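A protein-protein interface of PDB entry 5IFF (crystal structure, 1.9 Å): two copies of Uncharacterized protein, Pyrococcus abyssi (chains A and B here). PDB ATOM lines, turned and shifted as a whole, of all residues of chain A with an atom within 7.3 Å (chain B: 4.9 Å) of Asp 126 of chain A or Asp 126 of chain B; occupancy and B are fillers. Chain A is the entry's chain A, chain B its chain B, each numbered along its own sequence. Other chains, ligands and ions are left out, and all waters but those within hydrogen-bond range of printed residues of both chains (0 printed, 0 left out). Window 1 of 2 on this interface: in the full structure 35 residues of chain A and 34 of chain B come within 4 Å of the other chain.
The side-chain carboxylate (OE2) of Glu 125 of chain B is in salt-bridge range of the guanidinium group (NH1) of Arg 110 of chain A, at 2.9 Å.
The backbone NH (N) of Tyr 124 of chain A is in hydrogen-bond range of the backbone carbonyl oxygen (O) of Val 130 of chain B (2.7 Å).
The side-chain carboxylate of Glu 125 of chain A lies within salt-bridge range of the guanidinium group of Arg 110 of chain B, at 2.9 Å.
The backbone carbonyl oxygen of Tyr 128 of chain B is in hydrogen-bond range of the backbone NH of Asp 126 of chain A (2.8 Å).
O of Tyr 128 of chain A lies within hydrogen-bond range of N of Asp 126 of chain B (2.8 Å).
O of Val 130 of chain A lies within hydrogen-bond range of N of Tyr 124 of chain B (2.6 Å).
O of Asp 126 of chain B lies close to O of Asp 126 of chain A (3.5 Å).
Tyr 124 of chain A touches Tyr 128 of chain B, and with the chains exchanged Tyr 128 of chain A touches Tyr 124 of chain B.
Glu 125 of chain A touches Val 127 of chain B, and with the chains exchanged Val 127 of chain A touches Glu 125 of chain B.
Asp 126 of chain A touches its own counterpart, Asp 126 of chain B.
Asp 126 of chain A touches Val 127 of chain B, and with the chains exchanged Val 127 of chain A touches Asp 126 of chain B.
8 positions are printed for both chains.
NH2 of Arg 110 of chain A lies within salt-bridge range of OE2 of Glu 112 of chain A.
The backbone carbonyl oxygen (O) of Arg 110 of chain A sits at hydrogen-bond distance from the backbone NH (N) of Val 127 of chain A (2.8 Å).
The guanidinium group (NH2) of Arg 111 of chain A lies within salt-bridge range of the side-chain carboxylate (OD1) of Asp 126 of chain A, at 2.8 Å.
The backbone carbonyl oxygen (O) of Glu 125 of chain A lies within hydrogen-bond range of the backbone NH (N) of Glu 112 of chain A (2.8 Å).
The backbone NH of Val 127 of chain B is in hydrogen-bond range of the backbone carbonyl oxygen of Arg 110 of chain B, at 2.8 Å.
The side-chain carboxylate (OD1) of Asp 126 of chain B is in salt-bridge range of the guanidinium group (NE) of Arg 111 of chain B, at 2.8 Å.
Arg 111 of chain B touches Gly 35 of chain A (NH2 to O, 3.6 Å).
Arg 111 of chain B touches Ile 36 of chain A (CB to CG1, 3.9997 Å).
NH2 of Arg 111 of chain A touches CG2 of Val 130 of chain B (3.2 Å).
Tyr 124 of chain A touches Tyr 128 of chain B (O to O, 3.95 Å).
CD of Glu 125 of chain A touches CG1 of Val 127 of chain B, 3.5 Å away.
Val 127 of chain B touches Asp 126 of chain A.
CA of Val 127 of chain A touches O of Asp 126 of chain B, at 3.5 Å.
Tyr 124 of chain B touches Tyr 128 of chain A (O to O, 3.8 Å).
Tyr 128 of chain A touches Tyr 128 of chain B (CD1 to CD1, 3.6 Å).
Val 130 of chain A touches Asp 126 of chain B.
Asp 126 of chain A touches just these residues of chain B: Asp 126 (3.5 Å), Val 127 (3.5 Å), Tyr 128 (2.8 Å) and Val 130 (3.4 Å).
Printed residues of chain A within 4 Å of Asp 126 of chain B: Asp 126, Val 127, Tyr 128 and Val 130.
Of the printed residues of chain B, Arg 110 of chain A touches Glu 125 (2.9 Å).
Printed residues of chain B within 4 Å of Arg 111 of chain A: Val 130.
Printed residues of chain A within 4 Å of Val 130 of chain B: Arg 111 (3.2 Å), Tyr 124 (2.7 Å) and Asp 126 (3.4 Å).
Printed residues of chain B within 4 Å of Gly 35 of chain A: Arg 111 (3.6 Å).
Glu 112 of chain A touches none of the printed residues of chain B.
The nearest residue of chain A that does not touch Asp 126 of chain B is Ile 36 of chain A (4.4 Å).
Hydrophobic or aromatic side chains of chain B within 4 Å of the printed part of chain A: Tyr 124, Val 127, Tyr 128 and Val 130.
Of the 16 printed residues of chain A, 12 touch a printed residue of chain B.
Hydrophobic or aromatic side chains of chain A that line the printed part of chain B: Ile 36, Pro 37, Tyr 124, Val 127, Tyr 128 and Val 130.
Among the printed residues, 24 pairs touch across the chains.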
ATOM      1  N   GLY A  35      18.230  22.042 -17.579  1.00  0.00           N
ATOM      2  CA  GLY A  35      17.518  20.930 -16.981  1.00  0.00           C
ATOM      3  C   GLY A  35      16.332  21.384 -16.153  1.00  0.00           C
ATOM      4  O   GLY A  35      16.096  22.582 -15.965  1.00  0.00           O
ATOM      5  N   ILE A  36      15.576  20.414 -15.654  1.00  0.00           N
ATOM      6  CA  ILE A  36      14.396  20.719 -14.857  1.00  0.00           C
ATOM      7  C   ILE A  36      14.852  21.219 -13.493  1.00  0.00           C
ATOM      8  O   ILE A  36      15.707  20.598 -12.867  1.00  0.00           O
ATOM      9  CB  ILE A  36      13.496  19.457 -14.698  1.00  0.00           C
ATOM     10  CG1 ILE A  36      13.330  18.762 -16.043  1.00  0.00           C
ATOM     11  CG2 ILE A  36      12.151  19.816 -14.109  1.00  0.00           C
ATOM     12  CD1 ILE A  36      12.666  17.433 -15.940  1.00  0.00           C
ATOM     13  N   PRO A  37      14.275  22.326 -13.011  1.00  0.00           N
ATOM     14  CA  PRO A  37      14.738  22.736 -11.678  1.00  0.00           C
ATOM     15  C   PRO A  37      14.485  21.646 -10.620  1.00  0.00           C
ATOM     16  O   PRO A  37      13.432  20.964 -10.651  1.00  0.00           O
ATOM     17  CB  PRO A  37      13.926  23.993 -11.400  1.00  0.00           C
ATOM     18  CG  PRO A  37      13.590  24.535 -12.794  1.00  0.00           C
ATOM     19  CD  PRO A  37      13.329  23.289 -13.605  1.00  0.00           C
ATOM     20  N   ILE A 109      -0.224  18.780 -24.841  1.00  0.00           N
ATOM     21  CA  ILE A 109       0.621  17.669 -24.431  1.00  0.00           C
ATOM     22  C   ILE A 109       0.430  16.494 -25.387  1.00  0.00           C
ATOM     23  O   ILE A 109      -0.704  16.130 -25.670  1.00  0.00           O
ATOM     24  CB  ILE A 109       0.259  17.264 -23.000  1.00  0.00           C
ATOM     25  CG1 ILE A 109       0.720  18.364 -22.035  1.00  0.00           C
ATOM     26  CG2 ILE A 109       0.844  15.920 -22.651  1.00  0.00           C
ATOM     27  CD1 ILE A 109      -0.256  18.710 -20.911  1.00  0.00           C
ATOM     28  N   ARG A 110       1.505  15.916 -25.917  1.00  0.00           N
ATOM     29  CA  ARG A 110       1.341  14.763 -26.812  1.00  0.00           C
ATOM     30  C   ARG A 110       1.981  13.466 -26.252  1.00  0.00           C
ATOM     31  O   ARG A 110       2.950  13.517 -25.495  1.00  0.00           O
ATOM     32  CB  ARG A 110       1.915  15.084 -28.193  1.00  0.00           C
ATOM     33  CG  ARG A 110       3.433  15.183 -28.267  1.00  0.00           C
ATOM     34  CD  ARG A 110       3.878  15.562 -29.678  1.00  0.00           C
ATOM     35  NE  ARG A 110       5.301  15.306 -29.920  1.00  0.00           N
ATOM     36  CZ  ARG A 110       6.268  16.208 -29.761  1.00  0.00           C
ATOM     37  NH1 ARG A 110       5.966  17.431 -29.351  1.00  0.00           N
ATOM     38  NH2 ARG A 110       7.536  15.887 -30.009  1.00  0.00           N
ATOM     39  N   ARG A 111       1.427  12.308 -26.610  1.00  0.00           N
ATOM     40  CA  ARG A 111       2.041  11.047 -26.204  1.00  0.00           C
ATOM     41  C   ARG A 111       2.665  10.394 -27.422  1.00  0.00           C
ATOM     42  O   ARG A 111       2.004  10.210 -28.440  1.00  0.00           O
ATOM     43  CB  ARG A 111       1.032  10.106 -25.545  1.00  0.00           C
ATOM     44  CG  ARG A 111       1.667   8.753 -25.134  1.00  0.00           C
ATOM     45  CD  ARG A 111       0.663   7.756 -24.614  1.00  0.00           C
ATOM     46  NE  ARG A 111      -0.009   8.159 -23.376  1.00  0.00           N
ATOM     47  CZ  ARG A 111       0.584   8.272 -22.194  1.00  0.00           C
ATOM     48  NH1 ARG A 111      -0.108   8.620 -21.118  1.00  0.00           N
ATOM     49  NH2 ARG A 111       1.879   8.045 -22.087  1.00  0.00           N
ATOM     50  N   GLU A 112       3.951  10.071 -27.327  1.00  0.00           N
ATOM     51  CA  GLU A 112       4.670   9.462 -28.434  1.00  0.00           C
ATOM     52  C   GLU A 112       4.950   8.018 -28.116  1.00  0.00           C
ATOM     53  O   GLU A 112       5.300   7.681 -26.985  1.00  0.00           O
ATOM     54  CB  GLU A 112       5.986  10.186 -28.719  1.00  0.00           C
ATOM     55  CG  GLU A 112       5.840  11.609 -29.269  1.00  0.00           C
ATOM     56  CD  GLU A 112       7.150  12.152 -29.841  1.00  0.00           C
ATOM     57  OE1 GLU A 112       8.179  11.441 -29.767  1.00  0.00           O
ATOM     58  OE2 GLU A 112       7.156  13.288 -30.363  1.00  0.00           O
ATOM     59  N   TYR A 124       5.975   4.446 -23.645  1.00  0.00           N
ATOM     60  CA  TYR A 124       5.509   5.653 -24.338  1.00  0.00           C
ATOM     61  C   TYR A 124       6.191   6.845 -23.690  1.00  0.00           C
ATOM     62  O   TYR A 124       6.792   6.712 -22.628  1.00  0.00           O
ATOM     63  CB  TYR A 124       3.985   5.813 -24.267  1.00  0.00           C
ATOM     64  CG  TYR A 124       3.252   4.742 -25.044  1.00  0.00           C
ATOM     65  CD1 TYR A 124       2.830   4.966 -26.346  1.00  0.00           C
ATOM     66  CD2 TYR A 124       3.024   3.479 -24.483  1.00  0.00           C
ATOM     67  CE1 TYR A 124       2.175   3.969 -27.065  1.00  0.00           C
ATOM     68  CE2 TYR A 124       2.376   2.483 -25.187  1.00  0.00           C
ATOM     69  CZ  TYR A 124       1.953   2.733 -26.478  1.00  0.00           C
ATOM     70  OH  TYR A 124       1.302   1.750 -27.192  1.00  0.00           O
ATOM     71  N   GLU A 125       6.120   8.004 -24.336  1.00  0.00           N
ATOM     72  CA  GLU A 125       6.654   9.216 -23.732  1.00  0.00           C
ATOM     73  C   GLU A 125       5.588  10.312 -23.768  1.00  0.00           C
ATOM     74  O   GLU A 125       5.036  10.585 -24.828  1.00  0.00           O
ATOM     75  CB  GLU A 125       7.935   9.647 -24.458  1.00  0.00           C
ATOM     76  CG  GLU A 125       9.184   8.887 -24.026  1.00  0.00           C
ATOM     77  CD  GLU A 125      10.452   9.211 -24.860  1.00  0.00           C
ATOM     78  OE1 GLU A 125      10.341   9.718 -26.000  1.00  0.00           O
ATOM     79  OE2 GLU A 125      11.571   8.947 -24.364  1.00  0.00           O
ATOM     80  N   ASP A 126       5.256  10.898 -22.613  1.00  0.00           N
ATOM     81  CA  ASP A 126       4.378  12.071 -22.574  1.00  0.00           C
ATOM     82  C   ASP A 126       5.235  13.341 -22.670  1.00  0.00           C
ATOM     83  O   ASP A 126       6.226  13.472 -21.946  1.00  0.00           O
ATOM     84  CB  ASP A 126       3.530  12.090 -21.305  1.00  0.00           C
ATOM     85  CG  ASP A 126       2.381  11.096 -21.363  1.00  0.00           C
ATOM     86  OD1 ASP A 126       1.903  10.821 -22.487  1.00  0.00           O
ATOM     87  OD2 ASP A 126       1.952  10.609 -20.294  1.00  0.00           O
ATOM     88  N   VAL A 127       4.848  14.275 -23.544  1.00  0.00           N
ATOM     89  CA  VAL A 127       5.753  15.354 -23.929  1.00  0.00           C
ATOM     90  C   VAL A 127       5.079  16.706 -23.661  1.00  0.00           C
ATOM     91  O   VAL A 127       4.043  17.005 -24.257  1.00  0.00           O
ATOM     92  CB  VAL A 127       6.177  15.263 -25.431  1.00  0.00           C
ATOM     93  CG1 VAL A 127       7.324  16.206 -25.721  1.00  0.00           C
ATOM     94  CG2 VAL A 127       6.569  13.822 -25.818  1.00  0.00           C
ATOM     95  N   TYR A 128       5.651  17.464 -22.729  1.00  0.00           N
ATOM     96  CA  TYR A 128       5.115  18.754 -22.282  1.00  0.00           C
ATOM     97  C   TYR A 128       5.935  19.918 -22.845  1.00  0.00           C
ATOM     98  O   TYR A 128       7.158  19.940 -22.693  1.00  0.00           O
ATOM     99  CB  TYR A 128       5.139  18.857 -20.764  1.00  0.00           C
ATOM    100  CG  TYR A 128       4.201  17.949 -20.027  1.00  0.00           C
ATOM    101  CD1 TYR A 128       4.433  16.570 -19.959  1.00  0.00           C
ATOM    102  CD2 TYR A 128       3.095  18.465 -19.365  1.00  0.00           C
ATOM    103  CE1 TYR A 128       3.566  15.738 -19.274  1.00  0.00           C
ATOM    104  CE2 TYR A 128       2.229  17.638 -18.673  1.00  0.00           C
ATOM    105  CZ  TYR A 128       2.476  16.276 -18.629  1.00  0.00           C
ATOM    106  OH  TYR A 128       1.616  15.464 -17.937  1.00  0.00           O
ATOM    107  N   PRO A 129       5.266  20.907 -23.464  1.00  0.00           N
ATOM    108  CA  PRO A 129       6.020  22.031 -24.028  1.00  0.00           C
ATOM    109  C   PRO A 129       6.415  23.022 -22.926  1.00  0.00           C
ATOM    110  O   PRO A 129       5.616  23.296 -22.016  1.00  0.00           O
ATOM    111  CB  PRO A 129       5.021  22.657 -25.014  1.00  0.00           C
ATOM    112  CG  PRO A 129       3.710  22.505 -24.279  1.00  0.00           C
ATOM    113  CD  PRO A 129       3.816  21.139 -23.540  1.00  0.00           C
ATOM    114  N   VAL A 130       7.637  23.538 -23.003  1.00  0.00           N
ATOM    115  CA  VAL A 130       8.123  24.551 -22.088  1.00  0.00           C
ATOM    116  C   VAL A 130       8.662  25.753 -22.871  1.00  0.00           C
ATOM    117  O   VAL A 130       9.439  25.583 -23.804  1.00  0.00           O
ATOM    118  CB  VAL A 130       9.222  23.964 -21.199  1.00  0.00           C
ATOM    119  CG1 VAL A 130       9.849  25.011 -20.303  1.00  0.00           C
ATOM    120  CG2 VAL A 130       8.648  22.803 -20.350  1.00  0.00           C
ATOM    121  N   VAL A 144       5.199  26.863 -18.264  1.00  0.00           N
ATOM    122  CA  VAL A 144       5.012  25.409 -18.342  1.00  0.00           C
ATOM    123  C   VAL A 144       3.511  25.134 -18.300  1.00  0.00           C
ATOM    124  O   VAL A 144       2.718  26.046 -18.014  1.00  0.00           O
ATOM    125  CB  VAL A 144       5.699  24.695 -17.188  1.00  0.00           C
ATOM    126  CG1 VAL A 144       7.221  24.889 -17.277  1.00  0.00           C
ATOM    127  CG2 VAL A 144       5.182  25.272 -15.881  1.00  0.00           C
ATOM    128  N   HIS A 147      -2.018  19.855 -16.239  1.00  0.00           N
ATOM    129  CA  HIS A 147      -3.391  19.465 -16.525  1.00  0.00           C
ATOM    130  C   HIS A 147      -4.298  20.217 -15.581  1.00  0.00           C
ATOM    131  O   HIS A 147      -3.913  20.480 -14.437  1.00  0.00           O
ATOM    132  CB  HIS A 147      -3.589  17.958 -16.393  1.00  0.00           C
ATOM    133  CG  HIS A 147      -3.251  17.214 -17.641  1.00  0.00           C
ATOM    134  ND1 HIS A 147      -2.205  16.315 -17.718  1.00  0.00           N
ATOM    135  CD2 HIS A 147      -3.804  17.254 -18.876  1.00  0.00           C
ATOM    136  CE1 HIS A 147      -2.141  15.822 -18.941  1.00  0.00           C
ATOM    137  NE2 HIS A 147      -3.101  16.377 -19.665  1.00  0.00           N
ATOM    138  N   ARG B 110      13.259  14.031 -18.524  1.00  0.00           N
ATOM    139  CA  ARG B 110      14.302  14.876 -19.114  1.00  0.00           C
ATOM    140  C   ARG B 110      13.778  16.116 -19.873  1.00  0.00           C
ATOM    141  O   ARG B 110      12.669  16.105 -20.427  1.00  0.00           O
ATOM    142  CB  ARG B 110      15.179  14.041 -20.054  1.00  0.00           C
ATOM    143  CG  ARG B 110      14.526  13.607 -21.366  1.00  0.00           C
ATOM    144  CD  ARG B 110      15.460  12.648 -22.122  1.00  0.00           C
ATOM    145  NE  ARG B 110      14.941  12.231 -23.428  1.00  0.00           N
ATOM    146  CZ  ARG B 110      14.048  11.256 -23.605  1.00  0.00           C
ATOM    147  NH1 ARG B 110      13.545  10.616 -22.554  1.00  0.00           N
ATOM    148  NH2 ARG B 110      13.638  10.936 -24.828  1.00  0.00           N
ATOM    149  N   ARG B 111      14.589  17.177 -19.892  1.00  0.00           N
ATOM    150  CA  ARG B 111      14.258  18.399 -20.637  1.00  0.00           C
ATOM    151  C   ARG B 111      15.095  18.506 -21.895  1.00  0.00           C
ATOM    152  O   ARG B 111      16.314  18.627 -21.824  1.00  0.00           O
ATOM    153  CB  ARG B 111      14.461  19.651 -19.775  1.00  0.00           C
ATOM    154  CG  ARG B 111      14.289  20.994 -20.533  1.00  0.00           C
ATOM    155  CD  ARG B 111      14.062  22.150 -19.546  1.00  0.00           C
ATOM    156  NE  ARG B 111      12.766  21.982 -18.906  1.00  0.00           N
ATOM    157  CZ  ARG B 111      12.287  22.745 -17.931  1.00  0.00           C
ATOM    158  NH1 ARG B 111      11.082  22.486 -17.439  1.00  0.00           N
ATOM    159  NH2 ARG B 111      13.002  23.766 -17.460  1.00  0.00           N
ATOM    160  N   TYR B 124      11.193  24.256 -25.257  1.00  0.00           N
ATOM    161  CA  TYR B 124      11.807  23.011 -24.799  1.00  0.00           C
ATOM    162  C   TYR B 124      10.694  21.992 -24.571  1.00  0.00           C
ATOM    163  O   TYR B 124       9.521  22.363 -24.478  1.00  0.00           O
ATOM    164  CB  TYR B 124      12.573  23.189 -23.491  1.00  0.00           C
ATOM    165  CG  TYR B 124      13.786  24.063 -23.564  1.00  0.00           C
ATOM    166  CD1 TYR B 124      13.672  25.454 -23.653  1.00  0.00           C
ATOM    167  CD2 TYR B 124      15.064  23.515 -23.515  1.00  0.00           C
ATOM    168  CE1 TYR B 124      14.802  26.277 -23.704  1.00  0.00           C
ATOM    169  CE2 TYR B 124      16.207  24.342 -23.573  1.00  0.00           C
ATOM    170  CZ  TYR B 124      16.054  25.708 -23.662  1.00  0.00           C
ATOM    171  OH  TYR B 124      17.145  26.522 -23.707  1.00  0.00           O
ATOM    172  N   GLU B 125      11.069  20.722 -24.458  1.00  0.00           N
ATOM    173  CA  GLU B 125      10.101  19.647 -24.248  1.00  0.00           C
ATOM    174  C   GLU B 125      10.490  18.813 -23.033  1.00  0.00           C
ATOM    175  O   GLU B 125      11.640  18.374 -22.911  1.00  0.00           O
ATOM    176  CB  GLU B 125       9.982  18.792 -25.517  1.00  0.00           C
ATOM    177  CG  GLU B 125       9.222  19.554 -26.640  1.00  0.00           C
ATOM    178  CD  GLU B 125       9.170  18.813 -27.972  1.00  0.00           C
ATOM    179  OE1 GLU B 125      10.018  17.950 -28.206  1.00  0.00           O
ATOM    180  OE2 GLU B 125       8.261  19.094 -28.784  1.00  0.00           O
ATOM    181  N   ASP B 126       9.568  18.664 -22.091  1.00  0.00           N
ATOM    182  CA  ASP B 126       9.836  17.826 -20.921  1.00  0.00           C
ATOM    183  C   ASP B 126       9.241  16.464 -21.219  1.00  0.00           C
ATOM    184  O   ASP B 126       8.072  16.383 -21.573  1.00  0.00           O
ATOM    185  CB  ASP B 126       9.245  18.407 -19.631  1.00  0.00           C
ATOM    186  CG  ASP B 126      10.014  19.625 -19.124  1.00  0.00           C
ATOM    187  OD1 ASP B 126      11.098  19.905 -19.680  1.00  0.00           O
ATOM    188  OD2 ASP B 126       9.564  20.260 -18.146  1.00  0.00           O
ATOM    189  N   VAL B 127      10.049  15.406 -21.083  1.00  0.00           N
ATOM    190  CA  VAL B 127       9.660  14.077 -21.548  1.00  0.00           C
ATOM    191  C   VAL B 127       9.496  13.095 -20.395  1.00  0.00           C
ATOM    192  O   VAL B 127      10.466  12.807 -19.687  1.00  0.00           O
ATOM    193  CB  VAL B 127      10.710  13.523 -22.516  1.00  0.00           C
ATOM    194  CG1 VAL B 127      10.255  12.211 -23.111  1.00  0.00           C
ATOM    195  CG2 VAL B 127      10.970  14.538 -23.609  1.00  0.00           C
ATOM    196  N   TYR B 128       8.275  12.595 -20.227  1.00  0.00           N
ATOM    197  CA  TYR B 128       7.916  11.715 -19.115  1.00  0.00           C
ATOM    198  C   TYR B 128       7.714  10.295 -19.648  1.00  0.00           C
ATOM    199  O   TYR B 128       6.927  10.090 -20.578  1.00  0.00           O
ATOM    200  CB  TYR B 128       6.631  12.180 -18.422  1.00  0.00           C
ATOM    201  CG  TYR B 128       6.733  13.444 -17.582  1.00  0.00           C
ATOM    202  CD1 TYR B 128       6.970  14.693 -18.173  1.00  0.00           C
ATOM    203  CD2 TYR B 128       6.561  13.395 -16.200  1.00  0.00           C
ATOM    204  CE1 TYR B 128       7.040  15.848 -17.395  1.00  0.00           C
ATOM    205  CE2 TYR B 128       6.633  14.537 -15.427  1.00  0.00           C
ATOM    206  CZ  TYR B 128       6.875  15.759 -16.029  1.00  0.00           C
ATOM    207  OH  TYR B 128       6.941  16.883 -15.238  1.00  0.00           O
ATOM    208  N   VAL B 130       6.339   6.461 -19.838  1.00  0.00           N
ATOM    209  CA  VAL B 130       5.146   5.739 -19.425  1.00  0.00           C
ATOM    210  C   VAL B 130       5.240   4.287 -19.879  1.00  0.00           C
ATOM    211  O   VAL B 130       5.528   4.040 -21.037  1.00  0.00           O
ATOM    212  CB  VAL B 130       3.889   6.361 -20.008  1.00  0.00           C
ATOM    213  CG1 VAL B 130       2.681   5.551 -19.625  1.00  0.00           C
ATOM    214  CG2 VAL B 130       3.726   7.796 -19.495  1.00  0.00           C
